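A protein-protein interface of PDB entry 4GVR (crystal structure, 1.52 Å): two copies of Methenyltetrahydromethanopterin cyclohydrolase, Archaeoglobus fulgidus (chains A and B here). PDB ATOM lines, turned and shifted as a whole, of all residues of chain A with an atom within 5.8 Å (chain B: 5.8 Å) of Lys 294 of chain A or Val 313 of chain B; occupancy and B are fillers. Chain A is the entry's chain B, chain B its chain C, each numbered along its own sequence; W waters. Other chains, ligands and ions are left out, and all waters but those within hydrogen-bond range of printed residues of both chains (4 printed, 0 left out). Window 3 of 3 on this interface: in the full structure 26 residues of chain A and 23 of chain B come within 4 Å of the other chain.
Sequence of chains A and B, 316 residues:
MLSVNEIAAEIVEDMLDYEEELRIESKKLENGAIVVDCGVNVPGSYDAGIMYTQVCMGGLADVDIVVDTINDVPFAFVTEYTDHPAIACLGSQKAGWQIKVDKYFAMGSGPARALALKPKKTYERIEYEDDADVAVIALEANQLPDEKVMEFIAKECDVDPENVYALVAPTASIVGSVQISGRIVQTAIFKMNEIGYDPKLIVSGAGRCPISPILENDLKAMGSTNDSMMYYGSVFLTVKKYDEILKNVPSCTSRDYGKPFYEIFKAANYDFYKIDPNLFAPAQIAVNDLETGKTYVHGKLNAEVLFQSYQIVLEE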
ATOM      1  N   VAL A 287     -20.730  21.428 -14.712  1.00  0.00           N
ATOM      2  CA  VAL A 287     -22.146  21.521 -15.087  1.00  0.00           C
ATOM      3  C   VAL A 287     -22.688  20.139 -15.397  1.00  0.00           C
ATOM      4  O   VAL A 287     -22.316  19.503 -16.400  1.00  0.00           O
ATOM      5  CB  VAL A 287     -22.329  22.417 -16.335  1.00  0.00           C
ATOM      6  CG1 VAL A 287     -23.790  22.503 -16.757  1.00  0.00           C
ATOM      7  CG2 VAL A 287     -21.674  23.812 -16.131  1.00  0.00           C
ATOM      8  N   ASN A 288     -23.648  19.709 -14.556  1.00  0.00           N
ATOM      9  CA  ASN A 288     -24.135  18.379 -14.710  1.00  0.00           C
ATOM     10  C   ASN A 288     -25.377  18.528 -15.572  1.00  0.00           C
ATOM     11  O   ASN A 288     -26.383  19.195 -15.182  1.00  0.00           O
ATOM     12  CB  ASN A 288     -24.560  17.857 -13.321  1.00  0.00           C
ATOM     13  CG  ASN A 288     -25.358  16.538 -13.330  1.00  0.00           C
ATOM     14  OD1 ASN A 288     -25.348  15.706 -14.261  1.00  0.00           O
ATOM     15  ND2 ASN A 288     -26.008  16.328 -12.225  1.00  0.00           N
ATOM     16  N   ASP A 289     -25.323  17.859 -16.712  1.00  0.00           N
ATOM     17  CA  ASP A 289     -26.356  17.943 -17.724  1.00  0.00           C
ATOM     18  C   ASP A 289     -27.338  16.794 -17.547  1.00  0.00           C
ATOM     19  O   ASP A 289     -26.971  15.639 -17.762  1.00  0.00           O
ATOM     20  CB  ASP A 289     -25.746  17.760 -19.127  1.00  0.00           C
ATOM     21  CG  ASP A 289     -26.765  17.798 -20.231  1.00  0.00           C
ATOM     22  OD1 ASP A 289     -27.944  18.276 -19.980  1.00  0.00           O
ATOM     23  OD2 ASP A 289     -26.418  17.291 -21.324  1.00  0.00           O
ATOM     24  N   LEU A 290     -28.590  17.091 -17.185  1.00  0.00           N
ATOM     25  CA  LEU A 290     -29.544  15.993 -16.948  1.00  0.00           C
ATOM     26  C   LEU A 290     -29.852  15.231 -18.242  1.00  0.00           C
ATOM     27  O   LEU A 290     -30.169  14.015 -18.221  1.00  0.00           O
ATOM     28  CB  LEU A 290     -30.809  16.576 -16.341  1.00  0.00           C
ATOM     29  CG  LEU A 290     -30.630  17.152 -14.927  1.00  0.00           C
ATOM     30  CD1 LEU A 290     -31.976  17.663 -14.407  1.00  0.00           C
ATOM     31  CD2 LEU A 290     -30.134  16.040 -13.994  1.00  0.00           C
ATOM     32  N   THR A 292     -27.875  14.405 -21.035  1.00  0.00           N
ATOM     33  CA  THR A 292     -26.927  13.382 -21.490  1.00  0.00           C
ATOM     34  C   THR A 292     -26.329  12.606 -20.306  1.00  0.00           C
ATOM     35  O   THR A 292     -25.627  11.574 -20.472  1.00  0.00           O
ATOM     36  CB  THR A 292     -25.754  14.033 -22.203  1.00  0.00           C
ATOM     37  OG1 THR A 292     -25.165  14.985 -21.309  1.00  0.00           O
ATOM     38  CG2 THR A 292     -26.203  14.714 -23.493  1.00  0.00           C
ATOM     39  N   GLY A 293     -26.527  13.150 -19.113  1.00  0.00           N
ATOM     40  CA  GLY A 293     -25.938  12.556 -17.906  1.00  0.00           C
ATOM     41  C   GLY A 293     -24.460  12.818 -17.716  1.00  0.00           C
ATOM     42  O   GLY A 293     -23.822  12.253 -16.808  1.00  0.00           O
ATOM     43  N   LYS A 294     -23.925  13.735 -18.512  1.00  0.00           N
ATOM     44  CA  LYS A 294     -22.513  14.062 -18.425  1.00  0.00           C
ATOM     45  C   LYS A 294     -22.311  15.310 -17.541  1.00  0.00           C
ATOM     46  O   LYS A 294     -23.210  16.159 -17.407  1.00  0.00           O
ATOM     47  CB  LYS A 294     -21.895  14.326 -19.830  1.00  0.00           C
ATOM     48  CG  LYS A 294     -21.878  13.113 -20.787  1.00  0.00           C
ATOM     49  CD  LYS A 294     -21.068  13.344 -22.071  1.00  0.00           C
ATOM     50  CE  LYS A 294     -21.129  12.088 -22.986  1.00  0.00           C
ATOM     51  NZ  LYS A 294     -20.254  12.146 -24.200  1.00  0.00           N
ATOM     52  N   THR A 295     -21.075  15.501 -17.055  1.00  0.00           N
ATOM     53  CA  THR A 295     -20.767  16.683 -16.283  1.00  0.00           C
ATOM     54  C   THR A 295     -19.519  17.411 -16.892  1.00  0.00           C
ATOM     55  O   THR A 295     -18.324  16.898 -16.966  1.00  0.00           O
ATOM     56  CB  THR A 295     -20.592  16.347 -14.778  1.00  0.00           C
ATOM     57  OG1 THR A 295     -21.873  15.982 -14.206  1.00  0.00           O
ATOM     58  CG2 THR A 295     -20.094  17.542 -13.970  1.00  0.00           C
ATOM     59  N   TYR A 296     -19.781  18.625 -17.380  1.00  0.00           N
ATOM     60  CA  TYR A 296     -18.751  19.350 -18.132  1.00  0.00           C
ATOM     61  C   TYR A 296     -18.017  20.322 -17.193  1.00  0.00           C
ATOM     62  O   TYR A 296     -18.668  21.139 -16.537  1.00  0.00           O
ATOM     63  CB  TYR A 296     -19.434  20.127 -19.262  1.00  0.00           C
ATOM     64  CG  TYR A 296     -20.096  19.260 -20.303  1.00  0.00           C
ATOM     65  CD1 TYR A 296     -21.416  18.808 -20.134  1.00  0.00           C
ATOM     66  CD2 TYR A 296     -19.398  18.868 -21.452  1.00  0.00           C
ATOM     67  CE1 TYR A 296     -22.039  18.015 -21.087  1.00  0.00           C
ATOM     68  CE2 TYR A 296     -19.999  18.088 -22.422  1.00  0.00           C
ATOM     69  CZ  TYR A 296     -21.328  17.669 -22.249  1.00  0.00           C
ATOM     70  OH  TYR A 296     -21.920  16.868 -23.197  1.00  0.00           O
ATOM     71  N   VAL A 297     -16.670  20.290 -17.212  1.00  0.00           N
ATOM     72  CA  VAL A 297     -15.892  21.090 -16.285  1.00  0.00           C
ATOM     73  C   VAL A 297     -15.179  22.194 -17.101  1.00  0.00           C
ATOM     74  O   VAL A 297     -14.547  21.926 -18.183  1.00  0.00           O
ATOM     75  CB  VAL A 297     -14.821  20.228 -15.561  1.00  0.00           C
ATOM     76  CG1 VAL A 297     -13.941  21.083 -14.640  1.00  0.00           C
ATOM     77  CG2 VAL A 297     -15.461  19.027 -14.851  1.00  0.00           C
ATOM     78  N   ILE B 214     -26.235  13.647 -11.206  1.00  0.00           N
ATOM     79  CA  ILE B 214     -27.376  12.847 -11.645  1.00  0.00           C
ATOM     80  C   ILE B 214     -27.129  12.358 -13.067  1.00  0.00           C
ATOM     81  O   ILE B 214     -26.945  13.172 -14.000  1.00  0.00           O
ATOM     82  CB  ILE B 214     -28.699  13.643 -11.588  1.00  0.00           C
ATOM     83  CG1 ILE B 214     -28.915  14.239 -10.171  1.00  0.00           C
ATOM     84  CG2 ILE B 214     -29.833  12.758 -12.067  1.00  0.00           C
ATOM     85  CD1 ILE B 214     -30.076  15.223 -10.089  1.00  0.00           C
ATOM     86  N   LEU B 215     -27.057  11.040 -13.207  1.00  0.00           N
ATOM     87  CA  LEU B 215     -26.808  10.416 -14.501  1.00  0.00           C
ATOM     88  C   LEU B 215     -28.144  10.218 -15.223  1.00  0.00           C
ATOM     89  O   LEU B 215     -29.214  10.519 -14.642  1.00  0.00           O
ATOM     90  CB  LEU B 215     -26.009   9.127 -14.315  1.00  0.00           C
ATOM     91  CG  LEU B 215     -24.576   9.316 -13.755  1.00  0.00           C
ATOM     92  CD1 LEU B 215     -23.686   8.140 -14.156  1.00  0.00           C
ATOM     93  CD2 LEU B 215     -23.807  10.600 -13.935  1.00  0.00           C
ATOM     94  N   GLU B 216     -28.100   9.655 -16.435  1.00  0.00           N
ATOM     95  CA  GLU B 216     -29.221   9.728 -17.348  1.00  0.00           C
ATOM     96  C   GLU B 216     -30.360   8.690 -17.111  1.00  0.00           C
ATOM     97  O   GLU B 216     -31.401   8.773 -17.742  1.00  0.00           O
ATOM     98  CB  GLU B 216     -28.696   9.821 -18.814  1.00  0.00           C
ATOM     99  CG  GLU B 216     -28.118   8.537 -19.400  1.00  0.00           C
ATOM    100  CD  GLU B 216     -26.632   8.323 -19.140  1.00  0.00           C
ATOM    101  OE1 GLU B 216     -26.031   8.963 -18.243  1.00  0.00           O
ATOM    102  OE2 GLU B 216     -26.038   7.515 -19.872  1.00  0.00           O
ATOM    103  N   TYR B 310     -18.458   9.262 -12.952  1.00  0.00           N
ATOM    104  CA  TYR B 310     -19.229  10.520 -12.951  1.00  0.00           C
ATOM    105  C   TYR B 310     -19.452  11.074 -14.351  1.00  0.00           C
ATOM    106  O   TYR B 310     -20.061  12.117 -14.516  1.00  0.00           O
ATOM    107  CB  TYR B 310     -18.582  11.556 -12.033  1.00  0.00           C
ATOM    108  CG  TYR B 310     -18.843  11.401 -10.531  1.00  0.00           C
ATOM    109  CD1 TYR B 310     -19.468  10.254  -9.961  1.00  0.00           C
ATOM    110  CD2 TYR B 310     -18.389  12.414  -9.672  1.00  0.00           C
ATOM    111  CE1 TYR B 310     -19.640  10.211  -8.576  1.00  0.00           C
ATOM    112  CE2 TYR B 310     -18.564  12.372  -8.313  1.00  0.00           C
ATOM    113  CZ  TYR B 310     -19.224  11.282  -7.768  1.00  0.00           C
ATOM    114  OH  TYR B 310     -19.366  11.306  -6.389  1.00  0.00           O
ATOM    115  N   GLN B 311     -18.858  10.428 -15.357  1.00  0.00           N
ATOM    116  CA  GLN B 311     -19.033  10.837 -16.744  1.00  0.00           C
ATOM    117  C   GLN B 311     -18.603  12.320 -16.878  1.00  0.00           C
ATOM    118  O   GLN B 311     -19.281  13.144 -17.535  1.00  0.00           O
ATOM    119  CB  GLN B 311     -20.461  10.577 -17.232  1.00  0.00           C
ATOM    120  CG  GLN B 311     -20.800   9.108 -17.157  1.00  0.00           C
ATOM    121  CD  GLN B 311     -22.171   8.737 -17.697  1.00  0.00           C
ATOM    122  OE1 GLN B 311     -23.146   9.529 -17.668  1.00  0.00           O
ATOM    123  NE2 GLN B 311     -22.279   7.496 -18.115  1.00  0.00           N
ATOM    124  N   ILE B 312     -17.500  12.632 -16.168  1.00  0.00           N
ATOM    125  CA  ILE B 312     -16.798  13.932 -16.300  1.00  0.00           C
ATOM    126  C   ILE B 312     -16.213  14.180 -17.698  1.00  0.00           C
ATOM    127  O   ILE B 312     -15.539  13.311 -18.280  1.00  0.00           O
ATOM    128  CB  ILE B 312     -15.658  14.063 -15.255  1.00  0.00           C
ATOM    129  CG1 ILE B 312     -16.180  14.010 -13.806  1.00  0.00           C
ATOM    130  CG2 ILE B 312     -14.835  15.308 -15.535  1.00  0.00           C
ATOM    131  CD1 ILE B 312     -17.142  15.123 -13.436  1.00  0.00           C
ATOM    132  N   VAL B 313     -16.495  15.364 -18.232  1.00  0.00           N
ATOM    133  CA  VAL B 313     -15.886  15.810 -19.528  1.00  0.00           C
ATOM    134  C   VAL B 313     -14.960  16.986 -19.241  1.00  0.00           C
ATOM    135  O   VAL B 313     -15.432  18.062 -18.857  1.00  0.00           O
ATOM    136  CB  VAL B 313     -16.974  16.180 -20.584  1.00  0.00           C
ATOM    137  CG1 VAL B 313     -16.317  16.623 -21.919  1.00  0.00           C
ATOM    138  CG2 VAL B 313     -17.930  15.001 -20.789  1.00  0.00           C
ATOM    139  N   LEU B 314     -13.639  16.827 -19.448  1.00  0.00           N
ATOM    140  CA  LEU B 314     -12.763  17.938 -19.219  1.00  0.00           C
ATOM    141  C   LEU B 314     -12.498  18.517 -20.582  1.00  0.00           C
ATOM    142  O   LEU B 314     -12.802  17.870 -21.591  1.00  0.00           O
ATOM    143  CB  LEU B 314     -11.463  17.480 -18.551  1.00  0.00           C
ATOM    144  CG  LEU B 314     -11.519  16.716 -17.215  1.00  0.00           C
ATOM    145  CD1 LEU B 314     -10.118  16.286 -16.754  1.00  0.00           C
ATOM    146  CD2 LEU B 314     -12.221  17.582 -16.170  1.00  0.00           C
ATOM    147  N   GLU B 315     -11.884  19.696 -20.639  1.00  0.00           N
ATOM    148  CA  GLU B 315     -11.634  20.392 -21.925  1.00  0.00           C
ATOM    149  C   GLU B 315     -10.453  19.882 -22.796  1.00  0.00           C
ATOM    150  O   GLU B 315      -9.545  19.231 -22.290  1.00  0.00           O
ATOM    151  CB  GLU B 315     -11.466  21.875 -21.662  1.00  0.00           C
ATOM    152  CG  GLU B 315     -12.762  22.613 -21.395  1.00  0.00           C
ATOM    153  CD  GLU B 315     -12.520  24.066 -21.022  1.00  0.00           C
ATOM    154  OE1 GLU B 315     -11.335  24.483 -20.926  1.00  0.00           O
ATOM    155  OE2 GLU B 315     -13.489  24.814 -20.816  1.00  0.00           O
HETATM  156  O   HOH W   1     -15.812  20.265 -20.461  1.00  0.00           O
HETATM  157  O   HOH W   2     -23.908   9.628 -21.184  1.00  0.00           O
HETATM  158  O   HOH W   3     -11.655  21.143 -18.243  1.00  0.00           O
HETATM  159  O   HOH W   4     -22.479  13.446 -14.706  1.00  0.00           O
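Printed residues of chain A that touch a printed residue of chain B: Asn 288, Leu 290, Thr 292, Gly 293, Lys 294, Thr 295, Tyr 296 and Val 297.
Hydrophobic or aromatic side chains of chain A that line the printed part of chain B: Leu 290, Tyr 296 and Val 297.
Among the printed residues, 16 pairs touch across the chains.
OE1 of Gln 311 of chain B lies close to OE1 of Glu 216 of chain B (3.0 Å).
The side-chain carboxylate (OD2) of Asp 289 of chain A lies within hydrogen-bond range of the side-chain hydroxyl (OG1) of Thr 292 of chain A (2.6 Å).
The side-chain amide oxygen of Asn 288 of chain A lies close to the side-chain hydroxyl of Thr 295 of chain A (3.5 Å).
The backbone NH (N) of Asp 289 of chain A lies within hydrogen-bond range of the backbone carbonyl oxygen (O) of Lys 294 of chain A, 2.8 Å away.
The backbone NH (N) of Val 287 of chain A sits at hydrogen-bond distance from the backbone carbonyl oxygen (O) of Tyr 296 of chain A, 2.8 Å away.
N of Lys 294 of chain A lies close to OG1 of Thr 292 of chain A, at 3.3 Å.
Lys 294 of chain A touches just these residues of chain B: Gln 311 (3.5 Å) and Val 313 (3.8 Å).
Printed residues of chain B within 4 Å of Val 297 of chain A: Ile 312 (3.8 Å), Val 313 (3.0 Å), Leu 314 (3.8 Å) and Glu 315 (3.7 Å).
Of the printed residues of chain A, Glu 216 of chain B touches Thr 292 (3.5 Å) and Gly 293 (3.6 Å).
Of chain A, only Lys 294 (3.8 Å), Thr 295 (2.7 Å), Tyr 296 (3.6 Å) and Val 297 (3.0 Å) come within 4 Å of Val 313 of chain B.
No position is printed for both chains.
Of the 16 pairs that touch across the chains among the printed residues, none has its exchanged pair printed and touching as well.
Among the printed residues, pairs that only touch across the chains: Leu 290 of chain A with Ile 214 of chain B, Gly 293 of chain A with Leu 215 of chain B, Gly 293 of chain A with Glu 216 of chain B, Lys 294 of chain A with Gln 311 of chain B, Lys 294 of chain A with Val 313 of chain B, Thr 295 of chain A with Ile 312 of chain B, Tyr 296 of chain A with Val 313 of chain B, Val 297 of chain A with Ile 312 of chain B, Val 297 of chain A with Leu 314 of chain B and Val 297 of chain A with Glu 315 of chain B.
Water W4 lies within hydrogen-bond range of the side-chain hydroxyl (OG1) of Thr 295 of chain A (2.7 Å), the backbone carbonyl oxygen (O) of Gly 293 of chain A (2.8 Å) and the backbone carbonyl oxygen (O) of Tyr 310 of chain B (2.8 Å).
Water W2 lies within hydrogen-bond range of the backbone carbonyl oxygen (O) of Thr 292 of chain A (2.7 Å) and the side-chain carboxylate (OE2) of Glu 216 of chain B (3.3 Å).
Water W1 lies within hydrogen-bond range of O of Val 313 of chain B and O of Val 297 of chain A.
Water W3 lies within hydrogen-bond range of N of Glu 315 of chain B and O of Val 297 of chain A.
O of Thr 295 of chain A sits at hydrogen-bond distance from N of Val 313 of chain B.
O of Val 313 of chain B sits at hydrogen-bond distance from N of Val 297 of chain A (3.0 Å).
The backbone carbonyl oxygen (O) of Gln 311 of chain B is in hydrogen-bond range of the backbone NH (N) of Thr 295 of chain A (3.0 Å).
The backbone carbonyl oxygen (O) of Thr 292 of chain A lies close to the side-chain carboxylate (OE1) of Glu 216 of chain B, at 3.5 Å.
O of Gly 293 of chain A lies close to OE1 of Gln 311 of chain B, 2.9 Å away.
The side-chain amide nitrogen (ND2) of Asn 288 of chain A sits close to the backbone NH (N) of Ile 214 of chain B.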
